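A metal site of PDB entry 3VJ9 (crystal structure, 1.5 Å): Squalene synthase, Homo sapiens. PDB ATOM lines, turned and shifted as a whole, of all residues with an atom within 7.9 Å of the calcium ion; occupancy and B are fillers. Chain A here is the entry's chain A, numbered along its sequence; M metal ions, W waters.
Water W3 lies within hydrogen-bond range of OD1 of Asp 57 (2.6 Å) and OD1 of Asp 53 (2.7 Å).
Within 4 Å of the calcium ion: Asp 53, Glu 56 and Asp 57.
Along chain A the residues within 4 Å of the calcium ion span positions 53 to 57.
OE2 of Glu 56 lies within hydrogen-bond range of OH of Tyr 144 (3.3 Å).
The side-chain carboxylate (OD1) of Asp 53 is in salt-bridge range of the guanidinium group (NH2) of Arg 50, 2.7 Å away.
The guanidinium group of Arg 201 sits close to the side-chain carboxylate of Asp 57, at 3.3 Å.
The calcium ion is bound by the side-chain carboxylate (OD2) of Asp 53, water W2, the side-chain carboxylate (OD2) of Asp 57, water W3, the side-chain carboxylate (OE1) of Glu 56 and water W1.
The calcium ion has six donor atoms within binding distance.
Slightly farther from the calcium ion lies OD1 of Asp 57 (3.0 Å).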
ATOM      1  N   LEU A  49       4.462   2.427 -19.689  1.00  0.00           N
ATOM      2  CA  LEU A  49       3.999   1.619 -18.539  1.00  0.00           C
ATOM      3  C   LEU A  49       5.163   1.155 -17.685  1.00  0.00           C
ATOM      4  O   LEU A  49       5.070   1.136 -16.451  1.00  0.00           O
ATOM      5  CB  LEU A  49       3.211   0.397 -19.003  1.00  0.00           C
ATOM      6  CG  LEU A  49       1.840   0.702 -19.625  1.00  0.00           C
ATOM      7  CD1 LEU A  49       1.275  -0.564 -20.289  1.00  0.00           C
ATOM      8  CD2 LEU A  49       0.877   1.269 -18.606  1.00  0.00           C
ATOM      9  N   ARG A  50       6.277   0.787 -18.330  1.00  0.00           N
ATOM     10  CA  ARG A  50       7.471   0.370 -17.603  1.00  0.00           C
ATOM     11  C   ARG A  50       7.995   1.530 -16.765  1.00  0.00           C
ATOM     12  O   ARG A  50       8.386   1.353 -15.604  1.00  0.00           O
ATOM     13  CB  ARG A  50       8.535  -0.097 -18.588  1.00  0.00           C
ATOM     14  CG  ARG A  50       9.707  -0.833 -17.958  1.00  0.00           C
ATOM     15  CD  ARG A  50       9.475  -2.346 -17.840  1.00  0.00           C
ATOM     16  NE  ARG A  50       8.282  -2.684 -17.077  1.00  0.00           N
ATOM     17  CZ  ARG A  50       8.233  -2.786 -15.755  1.00  0.00           C
ATOM     18  NH1 ARG A  50       9.316  -2.605 -14.999  1.00  0.00           N
ATOM     19  NH2 ARG A  50       7.077  -3.079 -15.169  1.00  0.00           N
ATOM     20  N   LEU A  52       6.285   4.080 -15.584  1.00  0.00           N
ATOM     21  CA  LEU A  52       5.331   4.309 -14.512  1.00  0.00           C
ATOM     22  C   LEU A  52       5.496   3.263 -13.401  1.00  0.00           C
ATOM     23  O   LEU A  52       5.535   3.611 -12.217  1.00  0.00           O
ATOM     24  CB  LEU A  52       3.907   4.327 -15.089  1.00  0.00           C
ATOM     25  CG  LEU A  52       2.729   4.581 -14.136  1.00  0.00           C
ATOM     26  CD1 LEU A  52       2.950   5.897 -13.383  1.00  0.00           C
ATOM     27  CD2 LEU A  52       1.413   4.601 -14.888  1.00  0.00           C
ATOM     28  N   ASP A  53       5.595   1.996 -13.776  1.00  0.00           N
ATOM     29  CA  ASP A  53       5.779   0.930 -12.804  1.00  0.00           C
ATOM     30  C   ASP A  53       7.093   1.033 -12.053  1.00  0.00           C
ATOM     31  O   ASP A  53       7.172   0.657 -10.871  1.00  0.00           O
ATOM     32  CB  ASP A  53       5.699  -0.442 -13.482  1.00  0.00           C
ATOM     33  CG  ASP A  53       5.775  -1.551 -12.463  1.00  0.00           C
ATOM     34  OD1 ASP A  53       6.633  -2.454 -12.609  1.00  0.00           O
ATOM     35  OD2 ASP A  53       5.018  -1.483 -11.475  1.00  0.00           O
ATOM     36  N   THR A  54       8.125   1.528 -12.739  1.00  0.00           N
ATOM     37  CA  THR A  54       9.436   1.695 -12.120  1.00  0.00           C
ATOM     38  C   THR A  54       9.326   2.713 -10.990  1.00  0.00           C
ATOM     39  O   THR A  54       9.899   2.501  -9.915  1.00  0.00           O
ATOM     40  CB  THR A  54      10.500   2.062 -13.177  1.00  0.00           C
ATOM     41  OG1 THR A  54      10.640   0.974 -14.103  1.00  0.00           O
ATOM     42  CG2 THR A  54      11.860   2.398 -12.566  1.00  0.00           C
ATOM     43  N   LEU A  55       8.587   3.796 -11.227  1.00  0.00           N
ATOM     44  CA  LEU A  55       8.294   4.741 -10.158  1.00  0.00           C
ATOM     45  C   LEU A  55       7.521   4.104  -8.999  1.00  0.00           C
ATOM     46  O   LEU A  55       7.896   4.310  -7.840  1.00  0.00           O
ATOM     47  CB  LEU A  55       7.536   5.955 -10.732  1.00  0.00           C
ATOM     48  CG  LEU A  55       8.301   6.824 -11.739  1.00  0.00           C
ATOM     49  CD1 LEU A  55       7.379   7.814 -12.470  1.00  0.00           C
ATOM     50  CD2 LEU A  55       9.437   7.592 -11.043  1.00  0.00           C
ATOM     51  N   GLU A  56       6.465   3.358  -9.294  1.00  0.00           N
ATOM     52  CA  GLU A  56       5.609   2.775  -8.250  1.00  0.00           C
ATOM     53  C   GLU A  56       6.452   1.883  -7.355  1.00  0.00           C
ATOM     54  O   GLU A  56       6.347   1.961  -6.135  1.00  0.00           O
ATOM     55  CB  GLU A  56       4.449   1.952  -8.841  1.00  0.00           C
ATOM     56  CG  GLU A  56       3.479   1.414  -7.773  1.00  0.00           C
ATOM     57  CD  GLU A  56       2.684   0.159  -8.156  1.00  0.00           C
ATOM     58  OE1 GLU A  56       2.950  -0.466  -9.210  1.00  0.00           O
ATOM     59  OE2 GLU A  56       1.777  -0.226  -7.384  1.00  0.00           O
ATOM     60  N   ASP A  57       7.283   1.054  -7.978  1.00  0.00           N
ATOM     61  CA  ASP A  57       8.032   0.008  -7.298  1.00  0.00           C
ATOM     62  C   ASP A  57       9.276   0.472  -6.548  1.00  0.00           C
ATOM     63  O   ASP A  57       9.820  -0.279  -5.719  1.00  0.00           O
ATOM     64  CB  ASP A  57       8.481  -1.032  -8.319  1.00  0.00           C
ATOM     65  CG  ASP A  57       7.339  -1.835  -8.863  1.00  0.00           C
ATOM     66  OD1 ASP A  57       7.584  -2.669  -9.751  1.00  0.00           O
ATOM     67  OD2 ASP A  57       6.183  -1.652  -8.422  1.00  0.00           O
ATOM     68  N   ASP A  58       9.739   1.682  -6.857  1.00  0.00           N
ATOM     69  CA  ASP A  58      11.009   2.122  -6.296  1.00  0.00           C
ATOM     70  C   ASP A  58      10.843   2.585  -4.864  1.00  0.00           C
ATOM     71  O   ASP A  58      10.322   3.671  -4.598  1.00  0.00           O
ATOM     72  CB  ASP A  58      11.620   3.236  -7.147  1.00  0.00           C
ATOM     73  CG  ASP A  58      13.100   3.453  -6.859  1.00  0.00           C
ATOM     74  OD1 ASP A  58      13.779   4.016  -7.739  1.00  0.00           O
ATOM     75  OD2 ASP A  58      13.588   3.077  -5.770  1.00  0.00           O
ATOM     76  N   MET A  59      11.302   1.757  -3.922  1.00  0.00           N
ATOM     77  CA  MET A  59      11.107   2.042  -2.506  1.00  0.00           C
ATOM     78  C   MET A  59      12.084   3.104  -2.005  1.00  0.00           C
ATOM     79  O   MET A  59      11.937   3.585  -0.885  1.00  0.00           O
ATOM     80  CB  MET A  59      11.148   0.746  -1.684  1.00  0.00           C
ATOM     81  CG  MET A  59      10.109  -0.294  -2.077  1.00  0.00           C
ATOM     82  SD  MET A  59       8.392   0.220  -1.845  1.00  0.00           S
ATOM     83  CE  MET A  59       7.881   0.693  -3.492  1.00  0.00           C
ATOM     84  N   MET A 127      -2.492   3.650  -8.585  1.00  0.00           N
ATOM     85  CA  MET A 127      -1.232   3.277  -7.935  1.00  0.00           C
ATOM     86  C   MET A 127      -0.970   4.123  -6.691  1.00  0.00           C
ATOM     87  O   MET A 127      -0.591   3.598  -5.645  1.00  0.00           O
ATOM     88  CB  MET A 127      -0.040   3.421  -8.888  1.00  0.00           C
ATOM     89  CG  MET A 127       0.073   2.338  -9.943  1.00  0.00           C
ATOM     90  SD  MET A 127       1.371   2.770 -11.117  1.00  0.00           S
ATOM     91  CE  MET A 127       1.696   1.198 -11.907  1.00  0.00           C
ATOM     92  N   TYR A 144      -7.134  -3.207  -6.979  1.00  0.00           N
ATOM     93  CA  TYR A 144      -5.691  -3.020  -7.148  1.00  0.00           C
ATOM     94  C   TYR A 144      -5.248  -3.626  -8.479  1.00  0.00           C
ATOM     95  O   TYR A 144      -4.529  -2.993  -9.261  1.00  0.00           O
ATOM     96  CB  TYR A 144      -4.898  -3.677  -6.016  1.00  0.00           C
ATOM     97  CG  TYR A 144      -3.400  -3.599  -6.259  1.00  0.00           C
ATOM     98  CD1 TYR A 144      -2.732  -2.389  -6.096  1.00  0.00           C
ATOM     99  CD2 TYR A 144      -2.678  -4.695  -6.721  1.00  0.00           C
ATOM    100  CE1 TYR A 144      -1.365  -2.277  -6.359  1.00  0.00           C
ATOM    101  CE2 TYR A 144      -1.319  -4.590  -6.993  1.00  0.00           C
ATOM    102  CZ  TYR A 144      -0.668  -3.392  -6.803  1.00  0.00           C
ATOM    103  OH  TYR A 144       0.658  -3.268  -7.095  1.00  0.00           O
ATOM    104  N   VAL A 148      -3.296  -1.756 -11.862  1.00  0.00           N
ATOM    105  CA  VAL A 148      -1.951  -2.056 -12.337  1.00  0.00           C
ATOM    106  C   VAL A 148      -1.888  -3.015 -13.531  1.00  0.00           C
ATOM    107  O   VAL A 148      -0.827  -3.174 -14.143  1.00  0.00           O
ATOM    108  CB  VAL A 148      -1.026  -2.520 -11.197  1.00  0.00           C
ATOM    109  CG1 VAL A 148      -1.053  -1.521 -10.038  1.00  0.00           C
ATOM    110  CG2 VAL A 148      -1.401  -3.926 -10.723  1.00  0.00           C
ATOM    111  N   GLN A 185      -2.153 -10.695 -13.338  1.00  0.00           N
ATOM    112  CA  GLN A 185      -1.670  -9.990 -12.138  1.00  0.00           C
ATOM    113  C   GLN A 185      -1.880 -10.825 -10.884  1.00  0.00           C
ATOM    114  O   GLN A 185      -1.021 -10.866 -10.000  1.00  0.00           O
ATOM    115  CB  GLN A 185      -2.300  -8.611 -11.985  1.00  0.00           C
ATOM    116  CG  GLN A 185      -1.613  -7.807 -10.891  1.00  0.00           C
ATOM    117  CD  GLN A 185      -0.163  -7.542 -11.227  1.00  0.00           C
ATOM    118  OE1 GLN A 185       0.173  -7.249 -12.364  1.00  0.00           O
ATOM    119  NE2 GLN A 185       0.716  -7.634 -10.236  1.00  0.00           N
ATOM    120  N   ARG A 201       6.313  -5.517   0.966  1.00  0.00           N
ATOM    121  CA  ARG A 201       5.055  -5.270   0.274  1.00  0.00           C
ATOM    122  C   ARG A 201       4.053  -6.404   0.527  1.00  0.00           C
ATOM    123  O   ARG A 201       4.444  -7.568   0.602  1.00  0.00           O
ATOM    124  CB  ARG A 201       5.313  -5.129  -1.235  1.00  0.00           C
ATOM    125  CG  ARG A 201       6.426  -4.161  -1.576  1.00  0.00           C
ATOM    126  CD  ARG A 201       5.908  -2.723  -1.696  1.00  0.00           C
ATOM    127  NE  ARG A 201       5.267  -2.504  -2.987  1.00  0.00           N
ATOM    128  CZ  ARG A 201       5.915  -2.323  -4.132  1.00  0.00           C
ATOM    129  NH1 ARG A 201       7.247  -2.325  -4.172  1.00  0.00           N
ATOM    130  NH2 ARG A 201       5.226  -2.125  -5.257  1.00  0.00           N
ATOM    131  N   PHE A 203       0.374  -7.866  -0.816  1.00  0.00           N
ATOM    132  CA  PHE A 203      -0.631  -7.805  -1.866  1.00  0.00           C
ATOM    133  C   PHE A 203      -1.735  -8.862  -1.733  1.00  0.00           C
ATOM    134  O   PHE A 203      -2.758  -8.760  -2.398  1.00  0.00           O
ATOM    135  CB  PHE A 203      -0.001  -7.886  -3.262  1.00  0.00           C
ATOM    136  CG  PHE A 203       0.949  -6.767  -3.555  1.00  0.00           C
ATOM    137  CD1 PHE A 203       0.461  -5.507  -3.861  1.00  0.00           C
ATOM    138  CD2 PHE A 203       2.321  -6.962  -3.525  1.00  0.00           C
ATOM    139  CE1 PHE A 203       1.320  -4.462  -4.119  1.00  0.00           C
ATOM    140  CE2 PHE A 203       3.194  -5.924  -3.812  1.00  0.00           C
ATOM    141  CZ  PHE A 203       2.690  -4.674  -4.106  1.00  0.00           C
HETATM  142 CA    CA M   1       4.582  -2.219  -9.618  1.00  0.00          CA
HETATM  143  O   HOH W   1       3.424  -4.516  -9.876  1.00  0.00           O
HETATM  144  O   HOH W   2       4.062  -3.350  -7.964  1.00  0.00           O
HETATM  145  O   HOH W   3       5.557  -4.042 -10.698  1.00  0.00           O
